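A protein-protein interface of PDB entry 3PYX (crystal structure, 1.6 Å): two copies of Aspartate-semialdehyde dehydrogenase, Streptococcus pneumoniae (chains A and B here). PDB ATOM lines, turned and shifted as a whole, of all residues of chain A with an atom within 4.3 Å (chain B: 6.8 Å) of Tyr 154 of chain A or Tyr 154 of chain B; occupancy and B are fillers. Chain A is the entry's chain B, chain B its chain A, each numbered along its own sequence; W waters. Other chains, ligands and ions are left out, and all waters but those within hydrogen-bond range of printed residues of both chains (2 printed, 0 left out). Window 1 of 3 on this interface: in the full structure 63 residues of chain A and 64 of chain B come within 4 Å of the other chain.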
ATOM      1  N   SER A 152      -0.878   7.811 -15.750  1.00  0.00           N
ATOM      2  CA  SER A 152      -2.261   7.332 -15.534  1.00  0.00           C
ATOM      3  C   SER A 152      -2.286   6.717 -14.139  1.00  0.00           C
ATOM      4  O   SER A 152      -1.479   5.848 -13.814  1.00  0.00           O
ATOM      5  CB  SER A 152      -2.662   6.323 -16.615  1.00  0.00           C
ATOM      6  OG  SER A 152      -2.783   6.957 -17.881  1.00  0.00           O
ATOM      7  N   THR A 153      -3.216   7.162 -13.288  1.00  0.00           N
ATOM      8  CA  THR A 153      -3.201   6.707 -11.911  1.00  0.00           C
ATOM      9  C   THR A 153      -4.271   5.657 -11.618  1.00  0.00           C
ATOM     10  O   THR A 153      -5.259   5.522 -12.363  1.00  0.00           O
ATOM     11  CB  THR A 153      -3.359   7.869 -10.892  1.00  0.00           C
ATOM     12  OG1 THR A 153      -4.713   8.352 -10.920  1.00  0.00           O
ATOM     13  CG2 THR A 153      -2.365   9.048 -11.173  1.00  0.00           C
ATOM     14  N   TYR A 154      -4.082   4.939 -10.518  1.00  0.00           N
ATOM     15  CA  TYR A 154      -4.952   3.854 -10.078  1.00  0.00           C
ATOM     16  C   TYR A 154      -5.123   4.123  -8.586  1.00  0.00           C
ATOM     17  O   TYR A 154      -4.404   3.577  -7.743  1.00  0.00           O
ATOM     18  CB  TYR A 154      -4.291   2.479 -10.301  1.00  0.00           C
ATOM     19  CG  TYR A 154      -3.969   2.128 -11.763  1.00  0.00           C
ATOM     20  CD1 TYR A 154      -4.577   1.024 -12.362  1.00  0.00           C
ATOM     21  CD2 TYR A 154      -3.027   2.880 -12.519  1.00  0.00           C
ATOM     22  CE1 TYR A 154      -4.283   0.669 -13.698  1.00  0.00           C
ATOM     23  CE2 TYR A 154      -2.759   2.554 -13.869  1.00  0.00           C
ATOM     24  CZ  TYR A 154      -3.389   1.450 -14.430  1.00  0.00           C
ATOM     25  OH  TYR A 154      -3.074   1.108 -15.736  1.00  0.00           O
ATOM     26  N   GLN A 155      -6.054   5.028  -8.263  1.00  0.00           N
ATOM     27  CA  GLN A 155      -6.093   5.592  -6.925  1.00  0.00           C
ATOM     28  C   GLN A 155      -7.085   4.928  -5.991  1.00  0.00           C
ATOM     29  O   GLN A 155      -8.209   4.601  -6.374  1.00  0.00           O
ATOM     30  CB  GLN A 155      -6.333   7.107  -6.979  1.00  0.00           C
ATOM     31  CG  GLN A 155      -5.093   7.840  -7.514  1.00  0.00           C
ATOM     32  CD  GLN A 155      -5.250   9.353  -7.702  1.00  0.00           C
ATOM     33  OE1 GLN A 155      -5.065   9.869  -8.807  1.00  0.00           O
ATOM     34  NE2 GLN A 155      -5.562  10.075  -6.621  1.00  0.00           N
ATOM     35  N   ALA A 156      -6.640   4.760  -4.754  1.00  0.00           N
ATOM     36  CA  ALA A 156      -7.430   4.162  -3.668  1.00  0.00           C
ATOM     37  C   ALA A 156      -8.473   5.124  -3.134  1.00  0.00           C
ATOM     38  O   ALA A 156      -8.292   6.335  -3.150  1.00  0.00           O
ATOM     39  CB  ALA A 156      -6.505   3.735  -2.520  1.00  0.00           C
ATOM     40  N   VAL A 244      -7.606   8.185 -12.053  1.00  0.00           N
ATOM     41  CA  VAL A 244      -8.728   7.230 -12.016  1.00  0.00           C
ATOM     42  C   VAL A 244      -8.837   6.604 -10.635  1.00  0.00           C
ATOM     43  O   VAL A 244      -7.836   6.171 -10.038  1.00  0.00           O
ATOM     44  CB  VAL A 244      -8.513   6.124 -13.069  1.00  0.00           C
ATOM     45  CG1 VAL A 244      -9.708   5.181 -13.103  1.00  0.00           C
ATOM     46  CG2 VAL A 244      -8.203   6.763 -14.492  1.00  0.00           C
ATOM     47  N   ILE A 246     -10.051   3.467  -8.422  1.00  0.00           N
ATOM     48  CA  ILE A 246     -10.336   2.022  -8.566  1.00  0.00           C
ATOM     49  C   ILE A 246     -10.751   1.432  -7.210  1.00  0.00           C
ATOM     50  O   ILE A 246     -10.584   2.114  -6.189  1.00  0.00           O
ATOM     51  CB  ILE A 246      -9.140   1.242  -9.223  1.00  0.00           C
ATOM     52  CG1 ILE A 246      -7.884   1.296  -8.329  1.00  0.00           C
ATOM     53  CG2 ILE A 246      -8.858   1.765 -10.627  1.00  0.00           C
ATOM     54  CD1 ILE A 246      -6.840   0.242  -8.695  1.00  0.00           C
ATOM     55  N   HIS A 252      -1.975   4.063  -3.575  1.00  0.00           N
ATOM     56  CA  HIS A 252      -2.134   4.479  -4.972  1.00  0.00           C
ATOM     57  C   HIS A 252      -1.092   3.800  -5.832  1.00  0.00           C
ATOM     58  O   HIS A 252       0.047   3.596  -5.400  1.00  0.00           O
ATOM     59  CB  HIS A 252      -1.924   5.979  -5.159  1.00  0.00           C
ATOM     60  CG  HIS A 252      -2.967   6.841  -4.516  1.00  0.00           C
ATOM     61  ND1 HIS A 252      -4.215   6.385  -4.146  1.00  0.00           N
ATOM     62  CD2 HIS A 252      -2.951   8.170  -4.245  1.00  0.00           C
ATOM     63  CE1 HIS A 252      -4.912   7.387  -3.637  1.00  0.00           C
ATOM     64  NE2 HIS A 252      -4.167   8.477  -3.676  1.00  0.00           N
ATOM     65  N   SER A 253      -1.486   3.456  -7.045  1.00  0.00           N
ATOM     66  CA  SER A 253      -0.522   2.958  -8.026  1.00  0.00           C
ATOM     67  C   SER A 253      -0.528   3.881  -9.237  1.00  0.00           C
ATOM     68  O   SER A 253      -1.539   4.500  -9.576  1.00  0.00           O
ATOM     69  CB  SER A 253      -0.889   1.527  -8.478  1.00  0.00           C
ATOM     70  OG  SER A 253      -1.175   0.646  -7.401  1.00  0.00           O
ATOM     71  N   SER A 255       0.950   4.281 -13.414  1.00  0.00           N
ATOM     72  CA  SER A 255       1.718   3.939 -14.614  1.00  0.00           C
ATOM     73  C   SER A 255       2.337   5.236 -15.113  1.00  0.00           C
ATOM     74  O   SER A 255       1.637   6.170 -15.527  1.00  0.00           O
ATOM     75  CB  SER A 255       0.789   3.289 -15.655  1.00  0.00           C
ATOM     76  OG  SER A 255       1.525   3.073 -16.846  1.00  0.00           O
ATOM     77  N   TRP A 320       6.192   1.617 -12.883  1.00  0.00           N
ATOM     78  CA  TRP A 320       5.005   1.405 -12.040  1.00  0.00           C
ATOM     79  C   TRP A 320       5.425   1.854 -10.638  1.00  0.00           C
ATOM     80  O   TRP A 320       6.408   1.369 -10.093  1.00  0.00           O
ATOM     81  CB  TRP A 320       4.668  -0.079 -12.051  1.00  0.00           C
ATOM     82  CG  TRP A 320       3.441  -0.514 -11.286  1.00  0.00           C
ATOM     83  CD1 TRP A 320       3.395  -1.343 -10.214  1.00  0.00           C
ATOM     84  CD2 TRP A 320       2.079  -0.221 -11.629  1.00  0.00           C
ATOM     85  NE1 TRP A 320       2.076  -1.548  -9.811  1.00  0.00           N
ATOM     86  CE2 TRP A 320       1.257  -0.881 -10.683  1.00  0.00           C
ATOM     87  CE3 TRP A 320       1.486   0.547 -12.637  1.00  0.00           C
ATOM     88  CZ2 TRP A 320      -0.132  -0.801 -10.713  1.00  0.00           C
ATOM     89  CZ3 TRP A 320       0.081   0.649 -12.661  1.00  0.00           C
ATOM     90  CH2 TRP A 320      -0.703  -0.037 -11.717  1.00  0.00           C
ATOM     91  N   VAL B 151      -0.538   3.423 -23.934  1.00  0.00           N
ATOM     92  CA  VAL B 151      -1.787   3.030 -23.270  1.00  0.00           C
ATOM     93  C   VAL B 151      -1.489   2.358 -21.940  1.00  0.00           C
ATOM     94  O   VAL B 151      -0.530   1.587 -21.814  1.00  0.00           O
ATOM     95  CB  VAL B 151      -2.661   2.107 -24.198  1.00  0.00           C
ATOM     96  CG1 VAL B 151      -1.848   0.890 -24.703  1.00  0.00           C
ATOM     97  CG2 VAL B 151      -3.989   1.664 -23.486  1.00  0.00           C
ATOM     98  N   SER B 152      -2.303   2.672 -20.925  1.00  0.00           N
ATOM     99  CA  SER B 152      -2.265   1.941 -19.679  1.00  0.00           C
ATOM    100  C   SER B 152      -3.650   1.370 -19.459  1.00  0.00           C
ATOM    101  O   SER B 152      -4.634   2.111 -19.555  1.00  0.00           O
ATOM    102  CB  SER B 152      -1.944   2.890 -18.531  1.00  0.00           C
ATOM    103  OG  SER B 152      -0.607   3.397 -18.661  1.00  0.00           O
ATOM    104  N   THR B 153      -3.724   0.083 -19.169  1.00  0.00           N
ATOM    105  CA  THR B 153      -5.023  -0.582 -19.117  1.00  0.00           C
ATOM    106  C   THR B 153      -5.460  -0.859 -17.690  1.00  0.00           C
ATOM    107  O   THR B 153      -4.641  -0.875 -16.762  1.00  0.00           O
ATOM    108  CB  THR B 153      -5.058  -1.914 -19.886  1.00  0.00           C
ATOM    109  OG1 THR B 153      -4.337  -2.899 -19.158  1.00  0.00           O
ATOM    110  CG2 THR B 153      -4.450  -1.782 -21.278  1.00  0.00           C
ATOM    111  N   TYR B 154      -6.768  -1.076 -17.543  1.00  0.00           N
ATOM    112  CA  TYR B 154      -7.439  -1.301 -16.264  1.00  0.00           C
ATOM    113  C   TYR B 154      -8.362  -2.480 -16.575  1.00  0.00           C
ATOM    114  O   TYR B 154      -9.551  -2.312 -16.893  1.00  0.00           O
ATOM    115  CB  TYR B 154      -8.261  -0.059 -15.856  1.00  0.00           C
ATOM    116  CG  TYR B 154      -7.463   1.241 -15.607  1.00  0.00           C
ATOM    117  CD1 TYR B 154      -7.402   1.809 -14.336  1.00  0.00           C
ATOM    118  CD2 TYR B 154      -6.830   1.927 -16.658  1.00  0.00           C
ATOM    119  CE1 TYR B 154      -6.713   3.020 -14.095  1.00  0.00           C
ATOM    120  CE2 TYR B 154      -6.114   3.111 -16.434  1.00  0.00           C
ATOM    121  CZ  TYR B 154      -6.055   3.650 -15.161  1.00  0.00           C
ATOM    122  OH  TYR B 154      -5.357   4.818 -14.984  1.00  0.00           O
ATOM    123  N   GLN B 155      -7.795  -3.682 -16.518  1.00  0.00           N
ATOM    124  CA  GLN B 155      -8.445  -4.856 -17.096  1.00  0.00           C
ATOM    125  C   GLN B 155      -9.213  -5.677 -16.073  1.00  0.00           C
ATOM    126  O   GLN B 155      -8.752  -5.887 -14.952  1.00  0.00           O
ATOM    127  CB  GLN B 155      -7.419  -5.708 -17.855  1.00  0.00           C
ATOM    128  CG  GLN B 155      -7.032  -5.010 -19.168  1.00  0.00           C
ATOM    129  CD  GLN B 155      -5.963  -5.753 -19.966  1.00  0.00           C
ATOM    130  OE1 GLN B 155      -4.908  -5.200 -20.247  1.00  0.00           O
ATOM    131  NE2 GLN B 155      -6.246  -6.995 -20.357  1.00  0.00           N
ATOM    132  N   ALA B 156     -10.415  -6.107 -16.471  1.00  0.00           N
ATOM    133  CA  ALA B 156     -11.271  -6.965 -15.651  1.00  0.00           C
ATOM    134  C   ALA B 156     -10.774  -8.398 -15.520  1.00  0.00           C
ATOM    135  O   ALA B 156     -10.155  -8.944 -16.453  1.00  0.00           O
ATOM    136  CB  ALA B 156     -12.688  -6.967 -16.258  1.00  0.00           C
ATOM    137  N   ALA B 205      -3.833  -3.844  -7.502  1.00  0.00           N
ATOM    138  CA  ALA B 205      -3.699  -3.575  -8.926  1.00  0.00           C
ATOM    139  C   ALA B 205      -2.445  -4.318  -9.334  1.00  0.00           C
ATOM    140  O   ALA B 205      -1.351  -4.034  -8.852  1.00  0.00           O
ATOM    141  CB  ALA B 205      -3.590  -2.084  -9.218  1.00  0.00           C
ATOM    142  N   ILE B 209      -0.291  -8.970 -16.886  1.00  0.00           N
ATOM    143  CA  ILE B 209      -1.282  -9.788 -17.575  1.00  0.00           C
ATOM    144  C   ILE B 209      -0.503 -10.641 -18.568  1.00  0.00           C
ATOM    145  O   ILE B 209       0.350 -10.123 -19.304  1.00  0.00           O
ATOM    146  CB  ILE B 209      -2.347  -8.911 -18.266  1.00  0.00           C
ATOM    147  CG1 ILE B 209      -3.074  -8.140 -17.153  1.00  0.00           C
ATOM    148  CG2 ILE B 209      -3.289  -9.758 -19.148  1.00  0.00           C
ATOM    149  CD1 ILE B 209      -4.222  -7.339 -17.549  1.00  0.00           C
ATOM    150  N   THR B 242       1.199  -0.658 -20.906  1.00  0.00           N
ATOM    151  CA  THR B 242       1.298  -1.195 -19.557  1.00  0.00           C
ATOM    152  C   THR B 242      -0.074  -1.790 -19.271  1.00  0.00           C
ATOM    153  O   THR B 242      -1.090  -1.061 -19.311  1.00  0.00           O
ATOM    154  CB  THR B 242       1.581  -0.098 -18.521  1.00  0.00           C
ATOM    155  OG1 THR B 242       2.787   0.607 -18.860  1.00  0.00           O
ATOM    156  CG2 THR B 242       1.717  -0.685 -17.117  1.00  0.00           C
ATOM    157  N   CYS B 243      -0.103  -3.084 -18.989  1.00  0.00           N
ATOM    158  CA  CYS B 243      -1.359  -3.798 -18.810  1.00  0.00           C
ATOM    159  C   CYS B 243      -1.524  -4.248 -17.372  1.00  0.00           C
ATOM    160  O   CYS B 243      -0.695  -4.995 -16.832  1.00  0.00           O
ATOM    161  CB  CYS B 243      -1.477  -4.972 -19.785  1.00  0.00           C
ATOM    162  SG  CYS B 243      -1.501  -4.438 -21.540  1.00  0.00           S
ATOM    163  N   VAL B 244      -2.608  -3.772 -16.751  1.00  0.00           N
ATOM    164  CA  VAL B 244      -2.798  -3.938 -15.313  1.00  0.00           C
ATOM    165  C   VAL B 244      -4.161  -4.557 -15.031  1.00  0.00           C
ATOM    166  O   VAL B 244      -5.176  -4.113 -15.617  1.00  0.00           O
ATOM    167  CB  VAL B 244      -2.736  -2.569 -14.584  1.00  0.00           C
ATOM    168  CG1 VAL B 244      -2.817  -2.746 -13.043  1.00  0.00           C
ATOM    169  CG2 VAL B 244      -1.459  -1.786 -14.977  1.00  0.00           C
ATOM    170  N   ARG B 245      -4.181  -5.559 -14.150  1.00  0.00           N
ATOM    171  CA  ARG B 245      -5.444  -6.148 -13.685  1.00  0.00           C
ATOM    172  C   ARG B 245      -5.930  -5.399 -12.469  1.00  0.00           C
ATOM    173  O   ARG B 245      -5.143  -5.124 -11.538  1.00  0.00           O
ATOM    174  CB  ARG B 245      -5.258  -7.628 -13.342  1.00  0.00           C
ATOM    175  CG  ARG B 245      -6.587  -8.415 -13.182  1.00  0.00           C
ATOM    176  CD  ARG B 245      -7.145  -8.858 -14.564  1.00  0.00           C
ATOM    177  NE  ARG B 245      -6.253  -9.814 -15.212  1.00  0.00           N
ATOM    178  CZ  ARG B 245      -6.442 -10.293 -16.442  1.00  0.00           C
ATOM    179  NH1 ARG B 245      -7.505  -9.903 -17.148  1.00  0.00           N
ATOM    180  NH2 ARG B 245      -5.570 -11.152 -16.969  1.00  0.00           N
ATOM    181  N   ILE B 246      -7.224  -5.097 -12.443  1.00  0.00           N
ATOM    182  CA  ILE B 246      -7.828  -4.420 -11.293  1.00  0.00           C
ATOM    183  C   ILE B 246      -9.057  -5.207 -10.837  1.00  0.00           C
ATOM    184  O   ILE B 246      -9.502  -6.112 -11.560  1.00  0.00           O
ATOM    185  CB  ILE B 246      -8.166  -2.925 -11.582  1.00  0.00           C
ATOM    186  CG1 ILE B 246      -9.243  -2.801 -12.670  1.00  0.00           C
ATOM    187  CG2 ILE B 246      -6.869  -2.109 -11.908  1.00  0.00           C
ATOM    188  CD1 ILE B 246      -9.902  -1.380 -12.696  1.00  0.00           C
ATOM    189  N   VAL B 248     -12.198  -5.624 -11.029  1.00  0.00           N
ATOM    190  CA  VAL B 248     -13.405  -5.420 -11.831  1.00  0.00           C
ATOM    191  C   VAL B 248     -13.707  -6.789 -12.433  1.00  0.00           C
ATOM    192  O   VAL B 248     -12.786  -7.473 -12.888  1.00  0.00           O
ATOM    193  CB  VAL B 248     -13.161  -4.353 -12.937  1.00  0.00           C
ATOM    194  CG1 VAL B 248     -14.321  -4.329 -13.977  1.00  0.00           C
ATOM    195  CG2 VAL B 248     -12.899  -2.968 -12.329  1.00  0.00           C
ATOM    196  N   ALA B 251     -15.559  -5.821 -18.105  1.00  0.00           N
ATOM    197  CA  ALA B 251     -15.315  -4.585 -18.878  1.00  0.00           C
ATOM    198  C   ALA B 251     -13.929  -4.021 -18.612  1.00  0.00           C
ATOM    199  O   ALA B 251     -13.557  -3.766 -17.445  1.00  0.00           O
ATOM    200  CB  ALA B 251     -16.404  -3.502 -18.671  1.00  0.00           C
ATOM    201  N   HIS B 252     -13.158  -3.857 -19.692  1.00  0.00           N
ATOM    202  CA  HIS B 252     -11.828  -3.248 -19.593  1.00  0.00           C
ATOM    203  C   HIS B 252     -11.893  -1.750 -19.823  1.00  0.00           C
ATOM    204  O   HIS B 252     -12.637  -1.263 -20.679  1.00  0.00           O
ATOM    205  CB  HIS B 252     -10.885  -3.803 -20.672  1.00  0.00           C
ATOM    206  CG  HIS B 252     -10.544  -5.250 -20.535  1.00  0.00           C
ATOM    207  ND1 HIS B 252     -10.672  -5.961 -19.363  1.00  0.00           N
ATOM    208  CD2 HIS B 252      -9.979  -6.102 -21.429  1.00  0.00           C
ATOM    209  CE1 HIS B 252     -10.253  -7.199 -19.550  1.00  0.00           C
ATOM    210  NE2 HIS B 252      -9.828  -7.310 -20.796  1.00  0.00           N
ATOM    211  N   SER B 253     -11.082  -1.004 -19.073  1.00  0.00           N
ATOM    212  CA  SER B 253     -10.951   0.422 -19.293  1.00  0.00           C
ATOM    213  C   SER B 253      -9.531   0.725 -19.713  1.00  0.00           C
ATOM    214  O   SER B 253      -8.618   0.013 -19.296  1.00  0.00           O
ATOM    215  CB  SER B 253     -11.289   1.221 -18.037  1.00  0.00           C
ATOM    216  OG  SER B 253     -12.549   0.804 -17.529  1.00  0.00           O
ATOM    217  N   GLU B 254      -9.346   1.759 -20.532  1.00  0.00           N
ATOM    218  CA  GLU B 254      -7.988   2.110 -21.001  1.00  0.00           C
ATOM    219  C   GLU B 254      -7.773   3.607 -20.998  1.00  0.00           C
ATOM    220  O   GLU B 254      -8.586   4.374 -21.541  1.00  0.00           O
ATOM    221  CB  GLU B 254      -7.741   1.562 -22.431  1.00  0.00           C
ATOM    222  CG  GLU B 254      -7.877   0.054 -22.511  1.00  0.00           C
ATOM    223  CD  GLU B 254      -7.896  -0.476 -23.925  1.00  0.00           C
ATOM    224  OE1 GLU B 254      -8.268   0.269 -24.849  1.00  0.00           O
ATOM    225  OE2 GLU B 254      -7.593  -1.679 -24.096  1.00  0.00           O
ATOM    226  N   SER B 255      -6.655   4.036 -20.411  1.00  0.00           N
ATOM    227  CA  SER B 255      -6.206   5.397 -20.545  1.00  0.00           C
ATOM    228  C   SER B 255      -5.281   5.429 -21.758  1.00  0.00           C
ATOM    229  O   SER B 255      -4.212   4.825 -21.737  1.00  0.00           O
ATOM    230  CB  SER B 255      -5.455   5.826 -19.276  1.00  0.00           C
ATOM    231  OG  SER B 255      -4.961   7.134 -19.446  1.00  0.00           O
ATOM    232  N   ALA B 293     -16.865   1.138 -16.660  1.00  0.00           N
ATOM    233  CA  ALA B 293     -16.947  -0.330 -16.718  1.00  0.00           C
ATOM    234  C   ALA B 293     -18.339  -0.847 -16.378  1.00  0.00           C
ATOM    235  O   ALA B 293     -18.897  -1.648 -17.122  1.00  0.00           O
ATOM    236  CB  ALA B 293     -15.894  -0.976 -15.786  1.00  0.00           C
ATOM    237  N   TRP B 320     -10.356   8.087 -22.730  1.00  0.00           N
ATOM    238  CA  TRP B 320     -10.685   6.978 -21.849  1.00  0.00           C
ATOM    239  C   TRP B 320     -11.614   6.060 -22.630  1.00  0.00           C
ATOM    240  O   TRP B 320     -12.655   6.510 -23.136  1.00  0.00           O
ATOM    241  CB  TRP B 320     -11.414   7.525 -20.617  1.00  0.00           C
ATOM    242  CG  TRP B 320     -11.817   6.535 -19.555  1.00  0.00           C
ATOM    243  CD1 TRP B 320     -13.104   6.199 -19.184  1.00  0.00           C
ATOM    244  CD2 TRP B 320     -10.948   5.816 -18.674  1.00  0.00           C
ATOM    245  NE1 TRP B 320     -13.075   5.301 -18.143  1.00  0.00           N
ATOM    246  CE2 TRP B 320     -11.761   5.058 -17.804  1.00  0.00           C
ATOM    247  CE3 TRP B 320      -9.548   5.755 -18.529  1.00  0.00           C
ATOM    248  CZ2 TRP B 320     -11.235   4.232 -16.793  1.00  0.00           C
ATOM    249  CZ3 TRP B 320      -9.021   4.911 -17.548  1.00  0.00           C
ATOM    250  CH2 TRP B 320      -9.858   4.160 -16.687  1.00  0.00           C
HETATM  251  O   HOH W   1      -0.727   6.084 -19.380  1.00  0.00           O
HETATM  252  O   HOH W   2      -0.355  -2.042  -7.309  1.00  0.00           O
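The side-chain hydroxyl (OH) of Tyr 154 of chain A lies within hydrogen-bond range of the backbone carbonyl oxygen (O) of Thr 153 of chain B (2.7 Å).
The side-chain hydroxyl (OG) of Ser 152 of chain A lies within hydrogen-bond range of the side-chain hydroxyl (OG) of Ser 255 of chain B (2.7 Å).
OG of Ser 255 of chain A sits at hydrogen-bond distance from OG of Ser 152 of chain B (2.8 Å).
OG1 of Thr 242 of chain B lies within hydrogen-bond range of OG of Ser 255 of chain A (3.4 Å).
OH of Tyr 154 of chain B is in hydrogen-bond range of O of Thr 153 of chain A (2.7 Å).
O of Thr 242 of chain B lies within hydrogen-bond range of N of Thr 153 of chain B, 2.9 Å away.
N of Gln 155 of chain B is in hydrogen-bond range of O of Val 244 of chain B, at 2.8 Å.
The backbone NH (N) of Ile 246 of chain B is in hydrogen-bond range of the backbone carbonyl oxygen (O) of Gln 155 of chain B (3.0 Å).
The backbone carbonyl oxygen of Gln 155 of chain A sits at hydrogen-bond distance from the backbone NH of Ile 246 of chain A, at 3.0 Å.
The backbone carbonyl oxygen (O) of Ser 253 of chain A lies within hydrogen-bond range of the backbone NH (N) of Tyr 154 of chain A (2.7 Å).
The backbone NH (N) of Gln 155 of chain A lies within hydrogen-bond range of the backbone carbonyl oxygen (O) of Val 244 of chain A.
Ser 152 of chain B touches Ser 152 of chain A (CB to CB, 3.997 Å).
Tyr 154 of chain B touches Ser 152 of chain A.
Tyr 154 of chain A touches Ser 152 of chain B (OH to CB, 3.5 Å).
Tyr 154 of chain A touches Tyr 154 of chain B.
Tyr 154 of chain A touches Val 244 of chain B (OH to CG2, 3.4 Å).
CG2 of Val 244 of chain A touches OH of Tyr 154 of chain B, 3.5 Å away.
CG2 of Val 244 of chain A touches CZ3 of Trp 320 of chain B (3.7 Å).
CG2 of Ile 246 of chain A touches CD1 of Tyr 154 of chain B, 3.98 Å away.
Trp 320 of chain A touches Ala 205 of chain B (CZ2 to O, 3.9 Å).
Val 244 of chain B touches Trp 320 of chain A (CG1 to CH2, 3.7 Å).
Of the printed residues of chain B, Ile 246 of chain A touches Tyr 154 and Ile 246.
Of the printed residues of chain B, Ser 255 of chain A touches Ser 152 (2.8 Å) and Thr 242 (3.4 Å).
Of the printed residues of chain A, Ser 152 of chain B touches Ser 152 (3.997 Å), Tyr 154 (3.5 Å) and Ser 255 (2.8 Å).
Of the printed residues of chain A, Tyr 154 of chain B touches Ser 152 (3.5 Å), Thr 153 (2.7 Å), Tyr 154 (3.4 Å), Val 244 (3.5 Å) and Ile 246 (3.98 Å).
Of the printed residues of chain A, Ile 246 of chain B touches Tyr 154 (3.9 Å) and Ile 246 (3.9 Å).
Of the printed residues of chain A, Ser 255 of chain B touches Ser 152 (2.7 Å).
The nearest printed residue of chain B that does not touch Trp 320 of chain A is Thr 242 of chain B (4.7 Å).
Of the 11 printed residues of chain A, 7 touch a printed residue of chain B.
Printed residues of chain A that touch a printed residue of chain B: Ser 152, Thr 153, Tyr 154, Val 244, Ile 246, Ser 255 and Trp 320.
Hydrophobic or aromatic side chains of chain A that line the printed part of chain B: Tyr 154, Val 244, Ile 246 and Trp 320.
Ser 152 of chain A touches Tyr 154 of chain B, and with the chains exchanged Tyr 154 of chain A touches Ser 152 of chain B.
Tyr 154 of chain B touches its own counterpart, Tyr 154 of chain A.
Tyr 154 of chain A touches Val 244 of chain B, and with the chains exchanged Val 244 of chain A touches Tyr 154 of chain B.
Val 244 of chain A touches Trp 320 of chain B, and with the chains exchanged Trp 320 of chain A touches Val 244 of chain B.
Water W1 bridges the side-chain hydroxyl (OG) of Ser 152 of chain A and the side-chain hydroxyl (OG) of Ser 152 of chain B.
Water W2 lies within hydrogen-bond range of the backbone carbonyl oxygen (O) of Ala 205 of chain B and the side-chain hydroxyl (OG) of Ser 253 of chain A.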
